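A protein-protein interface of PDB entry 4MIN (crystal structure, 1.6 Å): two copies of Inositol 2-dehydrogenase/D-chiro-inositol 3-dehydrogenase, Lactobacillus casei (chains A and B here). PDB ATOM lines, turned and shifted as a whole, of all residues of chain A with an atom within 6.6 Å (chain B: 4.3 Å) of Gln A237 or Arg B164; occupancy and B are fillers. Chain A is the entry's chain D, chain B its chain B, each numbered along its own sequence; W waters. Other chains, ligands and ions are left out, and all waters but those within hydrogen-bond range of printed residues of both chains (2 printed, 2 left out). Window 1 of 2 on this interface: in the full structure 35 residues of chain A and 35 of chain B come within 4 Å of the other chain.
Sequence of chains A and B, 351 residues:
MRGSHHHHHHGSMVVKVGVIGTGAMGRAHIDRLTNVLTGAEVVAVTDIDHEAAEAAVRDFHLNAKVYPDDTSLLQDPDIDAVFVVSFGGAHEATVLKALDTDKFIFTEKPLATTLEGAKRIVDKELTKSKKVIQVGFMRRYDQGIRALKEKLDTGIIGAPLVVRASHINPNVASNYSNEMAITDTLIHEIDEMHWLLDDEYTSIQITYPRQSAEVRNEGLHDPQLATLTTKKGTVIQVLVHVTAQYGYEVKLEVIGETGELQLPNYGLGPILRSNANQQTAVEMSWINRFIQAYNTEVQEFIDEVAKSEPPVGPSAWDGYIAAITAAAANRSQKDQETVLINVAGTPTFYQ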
ATOM      1  N   VAL A 162       1.716   0.798  15.650  1.00  0.00           N
ATOM      2  CA  VAL A 162       2.633   0.529  14.548  1.00  0.00           C
ATOM      3  C   VAL A 162       4.000   0.160  15.124  1.00  0.00           C
ATOM      4  O   VAL A 162       4.397   0.706  16.093  1.00  0.00           O
ATOM      5  CB  VAL A 162       2.802   1.757  13.619  1.00  0.00           C
ATOM      6  CG1 VAL A 162       3.863   1.504  12.586  1.00  0.00           C
ATOM      7  CG2 VAL A 162       1.519   2.084  12.911  1.00  0.00           C
ATOM      8  N   VAL A 163       4.659  -0.804  14.505  1.00  0.00           N
ATOM      9  CA  VAL A 163       6.006  -1.167  14.845  1.00  0.00           C
ATOM     10  C   VAL A 163       6.867  -0.952  13.610  1.00  0.00           C
ATOM     11  O   VAL A 163       6.517  -1.333  12.563  1.00  0.00           O
ATOM     12  CB  VAL A 163       6.151  -2.620  15.294  1.00  0.00           C
ATOM     13  CG1 VAL A 163       7.596  -2.939  15.602  1.00  0.00           C
ATOM     14  CG2 VAL A 163       5.329  -2.892  16.503  1.00  0.00           C
ATOM     15  N   ARG A 164       7.990  -0.288  13.805  1.00  0.00           N
ATOM     16  CA  ARG A 164       8.943  -0.147  12.757  1.00  0.00           C
ATOM     17  C   ARG A 164      10.263  -0.769  13.158  1.00  0.00           C
ATOM     18  O   ARG A 164      10.759  -0.514  14.190  1.00  0.00           O
ATOM     19  CB  ARG A 164       9.122   1.313  12.386  1.00  0.00           C
ATOM     20  CG  ARG A 164       7.977   1.813  11.635  1.00  0.00           C
ATOM     21  CD  ARG A 164       8.118   3.200  11.194  1.00  0.00           C
ATOM     22  NE  ARG A 164       7.560   3.387   9.882  1.00  0.00           N
ATOM     23  CZ  ARG A 164       7.624   4.524   9.228  1.00  0.00           C
ATOM     24  NH1 ARG A 164       8.205   5.565   9.766  1.00  0.00           N
ATOM     25  NH2 ARG A 164       7.107   4.604   8.055  1.00  0.00           N
ATOM     26  N   ALA A 165      10.787  -1.612  12.296  1.00  0.00           N
ATOM     27  CA  ALA A 165      11.986  -2.366  12.596  1.00  0.00           C
ATOM     28  C   ALA A 165      12.917  -2.442  11.400  1.00  0.00           C
ATOM     29  O   ALA A 165      12.489  -2.413  10.295  1.00  0.00           O
ATOM     30  CB  ALA A 165      11.631  -3.778  13.037  1.00  0.00           C
ATOM     31  N   SER A 166      14.195  -2.554  11.703  1.00  0.00           N
ATOM     32  CA  SER A 166      15.221  -2.798  10.710  1.00  0.00           C
ATOM     33  C   SER A 166      16.091  -3.974  11.100  1.00  0.00           C
ATOM     34  O   SER A 166      16.443  -4.130  12.223  1.00  0.00           O
ATOM     35  CB  SER A 166      16.123  -1.560  10.527  1.00  0.00           C
ATOM     36  OG  SER A 166      15.431  -0.444  10.078  1.00  0.00           O
ATOM     37  N   LEU A 225      11.053  -5.205   1.914  1.00  0.00           N
ATOM     38  CA  LEU A 225      10.154  -4.635   2.875  1.00  0.00           C
ATOM     39  C   LEU A 225       9.070  -5.642   3.221  1.00  0.00           C
ATOM     40  O   LEU A 225       8.455  -6.194   2.351  1.00  0.00           O
ATOM     41  CB  LEU A 225       9.531  -3.344   2.365  1.00  0.00           C
ATOM     42  CG  LEU A 225      10.496  -2.249   1.972  1.00  0.00           C
ATOM     43  CD1 LEU A 225       9.757  -1.167   1.286  1.00  0.00           C
ATOM     44  CD2 LEU A 225      11.166  -1.665   3.140  1.00  0.00           C
ATOM     45  N   ALA A 226       8.897  -5.856   4.509  1.00  0.00           N
ATOM     46  CA  ALA A 226       7.900  -6.751   5.028  1.00  0.00           C
ATOM     47  C   ALA A 226       6.876  -6.002   5.842  1.00  0.00           C
ATOM     48  O   ALA A 226       7.210  -5.327   6.737  1.00  0.00           O
ATOM     49  CB  ALA A 226       8.532  -7.761   5.852  1.00  0.00           C
ATOM     50  N   THR A 227       5.621  -6.139   5.470  1.00  0.00           N
ATOM     51  CA  THR A 227       4.538  -5.630   6.276  1.00  0.00           C
ATOM     52  C   THR A 227       3.731  -6.751   6.888  1.00  0.00           C
ATOM     53  O   THR A 227       3.202  -7.557   6.204  1.00  0.00           O
ATOM     54  CB  THR A 227       3.601  -4.763   5.449  1.00  0.00           C
ATOM     55  OG1 THR A 227       4.313  -3.661   4.899  1.00  0.00           O
ATOM     56  CG2 THR A 227       2.478  -4.231   6.298  1.00  0.00           C
ATOM     57  N   LEU A 228       3.676  -6.768   8.206  1.00  0.00           N
ATOM     58  CA  LEU A 228       2.916  -7.760   8.939  1.00  0.00           C
ATOM     59  C   LEU A 228       1.774  -7.097   9.705  1.00  0.00           C
ATOM     60  O   LEU A 228       1.931  -6.060  10.220  1.00  0.00           O
ATOM     61  CB  LEU A 228       3.785  -8.511   9.913  1.00  0.00           C
ATOM     62  CG  LEU A 228       4.955  -9.350   9.413  1.00  0.00           C
ATOM     63  CD1 LEU A 228       6.158  -8.543   9.292  1.00  0.00           C
ATOM     64  CD2 LEU A 228       5.225 -10.478  10.312  1.00  0.00           C
ATOM     65  N   VAL A 235       0.307  -2.821  12.937  1.00  0.00           N
ATOM     66  CA  VAL A 235       1.008  -2.994  11.691  1.00  0.00           C
ATOM     67  C   VAL A 235       2.506  -2.892  11.939  1.00  0.00           C
ATOM     68  O   VAL A 235       2.957  -1.966  12.517  1.00  0.00           O
ATOM     69  CB  VAL A 235       0.570  -1.981  10.620  1.00  0.00           C
ATOM     70  CG1 VAL A 235       1.366  -2.145   9.383  1.00  0.00           C
ATOM     71  CG2 VAL A 235      -0.893  -2.121  10.280  1.00  0.00           C
ATOM     72  N   ILE A 236       3.222  -3.885  11.458  1.00  0.00           N
ATOM     73  CA  ILE A 236       4.657  -3.942  11.574  1.00  0.00           C
ATOM     74  C   ILE A 236       5.317  -3.762  10.202  1.00  0.00           C
ATOM     75  O   ILE A 236       5.002  -4.450   9.316  1.00  0.00           O
ATOM     76  CB  ILE A 236       5.109  -5.279  12.173  1.00  0.00           C
ATOM     77  CG1 ILE A 236       4.426  -5.508  13.512  1.00  0.00           C
ATOM     78  CG2 ILE A 236       6.616  -5.291  12.324  1.00  0.00           C
ATOM     79  CD1 ILE A 236       3.830  -6.859  13.682  1.00  0.00           C
ATOM     80  N   GLN A 237       6.203  -2.783  10.100  1.00  0.00           N
ATOM     81  CA  GLN A 237       6.958  -2.526   8.898  1.00  0.00           C
ATOM     82  C   GLN A 237       8.423  -2.836   9.149  1.00  0.00           C
ATOM     83  O   GLN A 237       9.050  -2.144   9.893  1.00  0.00           O
ATOM     84  CB  GLN A 237       6.847  -1.048   8.491  1.00  0.00           C
ATOM     85  CG  GLN A 237       5.474  -0.615   8.041  1.00  0.00           C
ATOM     86  CD  GLN A 237       5.398   0.827   7.595  1.00  0.00           C
ATOM     87  OE1 GLN A 237       5.983   1.698   8.177  1.00  0.00           O
ATOM     88  NE2 GLN A 237       4.664   1.060   6.543  1.00  0.00           N
ATOM     89  N   VAL A 238       8.938  -3.887   8.524  1.00  0.00           N
ATOM     90  CA  VAL A 238      10.315  -4.285   8.689  1.00  0.00           C
ATOM     91  C   VAL A 238      11.085  -4.018   7.441  1.00  0.00           C
ATOM     92  O   VAL A 238      10.674  -4.347   6.401  1.00  0.00           O
ATOM     93  CB  VAL A 238      10.451  -5.775   8.969  1.00  0.00           C
ATOM     94  CG1 VAL A 238      11.873  -6.113   9.356  1.00  0.00           C
ATOM     95  CG2 VAL A 238       9.521  -6.186  10.089  1.00  0.00           C
ATOM     96  N   LEU A 239      12.222  -3.393   7.612  1.00  0.00           N
ATOM     97  CA  LEU A 239      13.204  -3.302   6.572  1.00  0.00           C
ATOM     98  C   LEU A 239      14.266  -4.382   6.763  1.00  0.00           C
ATOM     99  O   LEU A 239      14.862  -4.441   7.766  1.00  0.00           O
ATOM    100  CB  LEU A 239      13.888  -1.937   6.569  1.00  0.00           C
ATOM    101  CG  LEU A 239      15.148  -1.806   5.711  1.00  0.00           C
ATOM    102  CD1 LEU A 239      14.784  -1.754   4.291  1.00  0.00           C
ATOM    103  CD2 LEU A 239      15.848  -0.585   6.110  1.00  0.00           C
ATOM    104  N   VAL B 162      15.209   3.177  -0.055  1.00  0.00           N
ATOM    105  CA  VAL B 162      14.066   3.300   0.823  1.00  0.00           C
ATOM    106  C   VAL B 162      14.177   4.595   1.637  1.00  0.00           C
ATOM    107  O   VAL B 162      15.213   4.955   2.091  1.00  0.00           O
ATOM    108  CB  VAL B 162      13.959   2.125   1.795  1.00  0.00           C
ATOM    109  CG1 VAL B 162      12.724   2.235   2.617  1.00  0.00           C
ATOM    110  CG2 VAL B 162      13.858   0.844   1.080  1.00  0.00           C
ATOM    111  N   VAL B 163      13.048   5.267   1.798  1.00  0.00           N
ATOM    112  CA  VAL B 163      12.959   6.392   2.692  1.00  0.00           C
ATOM    113  C   VAL B 163      11.896   6.079   3.750  1.00  0.00           C
ATOM    114  O   VAL B 163      10.831   5.649   3.415  1.00  0.00           O
ATOM    115  CB  VAL B 163      12.532   7.662   1.940  1.00  0.00           C
ATOM    116  CG1 VAL B 163      12.448   8.809   2.853  1.00  0.00           C
ATOM    117  CG2 VAL B 163      13.522   7.969   0.897  1.00  0.00           C
ATOM    118  N   ARG B 164      12.253   6.269   5.011  1.00  0.00           N
ATOM    119  CA  ARG B 164      11.327   6.087   6.105  1.00  0.00           C
ATOM    120  C   ARG B 164      11.171   7.387   6.823  1.00  0.00           C
ATOM    121  O   ARG B 164      12.117   7.969   7.224  1.00  0.00           O
ATOM    122  CB  ARG B 164      11.825   5.063   7.075  1.00  0.00           C
ATOM    123  CG  ARG B 164      12.029   3.753   6.479  1.00  0.00           C
ATOM    124  CD  ARG B 164      12.349   2.684   7.493  1.00  0.00           C
ATOM    125  NE  ARG B 164      11.403   1.645   7.319  1.00  0.00           N
ATOM    126  CZ  ARG B 164      11.260   0.585   8.071  1.00  0.00           C
ATOM    127  NH1 ARG B 164      11.994   0.391   9.124  1.00  0.00           N
ATOM    128  NH2 ARG B 164      10.351  -0.281   7.710  1.00  0.00           N
ATOM    129  N   ALA B 165       9.939   7.832   6.966  1.00  0.00           N
ATOM    130  CA  ALA B 165       9.678   9.143   7.509  1.00  0.00           C
ATOM    131  C   ALA B 165       8.500   9.105   8.460  1.00  0.00           C
ATOM    132  O   ALA B 165       7.700   8.230   8.390  1.00  0.00           O
ATOM    133  CB  ALA B 165       9.411  10.094   6.424  1.00  0.00           C
ATOM    134  N   LEU B 225      -0.672   5.158   7.340  1.00  0.00           N
ATOM    135  CA  LEU B 225       0.557   4.829   6.694  1.00  0.00           C
ATOM    136  C   LEU B 225       0.482   5.119   5.217  1.00  0.00           C
ATOM    137  O   LEU B 225      -0.340   4.598   4.539  1.00  0.00           O
ATOM    138  CB  LEU B 225       0.905   3.360   6.909  1.00  0.00           C
ATOM    139  CG  LEU B 225       1.134   2.920   8.335  1.00  0.00           C
ATOM    140  CD1 LEU B 225       1.217   1.399   8.463  1.00  0.00           C
ATOM    141  CD2 LEU B 225       2.377   3.512   8.853  1.00  0.00           C
ATOM    142  N   GLN B 237       8.058   5.222   2.861  1.00  0.00           N
ATOM    143  CA  GLN B 237       7.114   4.863   3.900  1.00  0.00           C
ATOM    144  C   GLN B 237       6.983   5.986   4.932  1.00  0.00           C
ATOM    145  O   GLN B 237       7.869   6.227   5.678  1.00  0.00           O
ATOM    146  CB  GLN B 237       7.538   3.581   4.620  1.00  0.00           C
ATOM    147  CG  GLN B 237       7.617   2.358   3.783  1.00  0.00           C
ATOM    148  CD  GLN B 237       8.091   1.148   4.535  1.00  0.00           C
ATOM    149  OE1 GLN B 237       8.971   1.235   5.325  1.00  0.00           O
ATOM    150  NE2 GLN B 237       7.481   0.028   4.293  1.00  0.00           N
ATOM    151  N   LEU B 252      13.151  11.684   9.354  1.00  0.00           N
ATOM    152  CA  LEU B 252      13.509  11.364   8.004  1.00  0.00           C
ATOM    153  C   LEU B 252      14.755  10.489   7.965  1.00  0.00           C
ATOM    154  O   LEU B 252      15.767  10.854   8.492  1.00  0.00           O
ATOM    155  CB  LEU B 252      13.746  12.624   7.191  1.00  0.00           C
ATOM    156  CG  LEU B 252      14.187  12.477   5.743  1.00  0.00           C
ATOM    157  CD1 LEU B 252      13.157  11.825   4.868  1.00  0.00           C
ATOM    158  CD2 LEU B 252      14.513  13.780   5.183  1.00  0.00           C
ATOM    159  N   GLU B 253      14.608   9.315   7.349  1.00  0.00           N
ATOM    160  CA  GLU B 253      15.702   8.393   7.171  1.00  0.00           C
ATOM    161  C   GLU B 253      15.785   7.924   5.734  1.00  0.00           C
ATOM    162  O   GLU B 253      14.817   7.501   5.185  1.00  0.00           O
ATOM    163  CB  GLU B 253      15.503   7.195   8.073  1.00  0.00           C
ATOM    164  CG  GLU B 253      16.520   6.129   7.942  1.00  0.00           C
ATOM    165  CD  GLU B 253      16.212   4.964   8.846  1.00  0.00           C
ATOM    166  OE1 GLU B 253      15.080   4.866   9.296  1.00  0.00           O
ATOM    167  OE2 GLU B 253      17.115   4.181   9.134  1.00  0.00           O
HETATM  168  O   HOH W   1       8.338  -2.494   5.729  1.00  0.00           O
HETATM  169  O   HOH W   2      17.291   1.375   9.121  1.00  0.00           O
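O of Ala B165 is in hydrogen-bond range of NH1 of Arg A164, at 3.0 Å.
The backbone carbonyl oxygen (O) of Ala A165 sits at hydrogen-bond distance from the guanidinium group (NH1) of Arg B164 (3.1 Å).
NH2 of Arg A164 lies within hydrogen-bond range of O of Gln B237 (3.0 Å).
NH2 of Arg B164 sits at hydrogen-bond distance from O of Gln A237, at 3.2 Å.
OE1 of Gln B237 sits at hydrogen-bond distance from NH2 of Arg B164 (3.1 Å).
The backbone carbonyl oxygen of Gln B237 sits at hydrogen-bond distance from the backbone NH of Ala B165.
N of Val A163 is in hydrogen-bond range of O of Val A235, at 2.9 Å.
The backbone NH (N) of Ala A165 lies within hydrogen-bond range of the backbone carbonyl oxygen (O) of Gln A237.
The backbone carbonyl oxygen of Arg B164 lies within hydrogen-bond range of the backbone NH of Glu B253, at 2.8 Å.
O of Ala A165 lies within hydrogen-bond range of N of Leu A239.
NH1 of Arg B164 touches OG of Ser A166, at 3.7 Å.
CD1 of Leu A225 touches NE2 of Gln B237, at 3.96 Å.
Val A235 touches Leu B225 (CG1 to CD1, 3.7 Å).
Leu B225 touches Gln A237.
Gln A237 touches Gln B237 (NE2 to NE2, 3.8 Å).
Val A238 touches Arg B164 (C to NH2, 3.8 Å).
N of Leu A239 touches NH2 of Arg B164, at 3.6 Å.
Gln A237 touches just these residues of chain B: Arg B164 (3.2 Å), Leu B225 (3.96 Å) and Gln B237 (3.8 Å).
Printed residues of chain A within 4 Å of Arg B164: Ala A165, Ser A166, Gln A237, Val A238 and Leu A239.
Of the printed residues of chain B, Leu A239 touches Arg B164 (3.6 Å).
Of the printed residues of chain A, Ala B165 touches Arg A164 (3.0 Å).
Printed residues of chain A within 4 Å of Gln B237: Arg A164 (3.0 Å), Leu A225 (3.96 Å) and Gln A237 (3.8 Å).
Of the printed residues of chain A, Leu B225 touches Val A235 (3.7 Å) and Gln A237 (3.96 Å).
Ala A226 touches none of the printed residues of chain B.
The nearest printed residue of chain B that does not touch Gln A237 is Ala B165 (6.8 Å).
The nearest residue of chain A that does not touch Arg B164 is Arg A164 (4.4 Å).
Printed residues of chain B that touch a printed residue of chain A: Arg B164, Ala B165, Leu B225 and Gln B237.
Hydrophobic or aromatic side chains of chain B that line the printed part of chain A: Leu B225.
Of the 14 printed residues of chain A, 8 touch a printed residue of chain B.
Arg A164 touches Ala B165, and with the chains exchanged Ala A165 touches Arg B164.
Arg A164 touches Gln B237, and with the chains exchanged Gln A237 touches Arg B164.
Leu A225 touches Gln B237, and with the chains exchanged Gln A237 touches Leu B225.
Gln A237 touches its own counterpart, Gln B237.
Water W2 lies within hydrogen-bond range of the side-chain hydroxyl (OG) of Ser A166 (2.8 Å) and the side-chain carboxylate (OE2) of Glu B253 (2.8 Å).
Water W1 lies within hydrogen-bond range of the side-chain amide nitrogen (NE2) of Gln B237, the backbone carbonyl oxygen (O) of Val A238 and the backbone carbonyl oxygen (O) of Ala A226.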
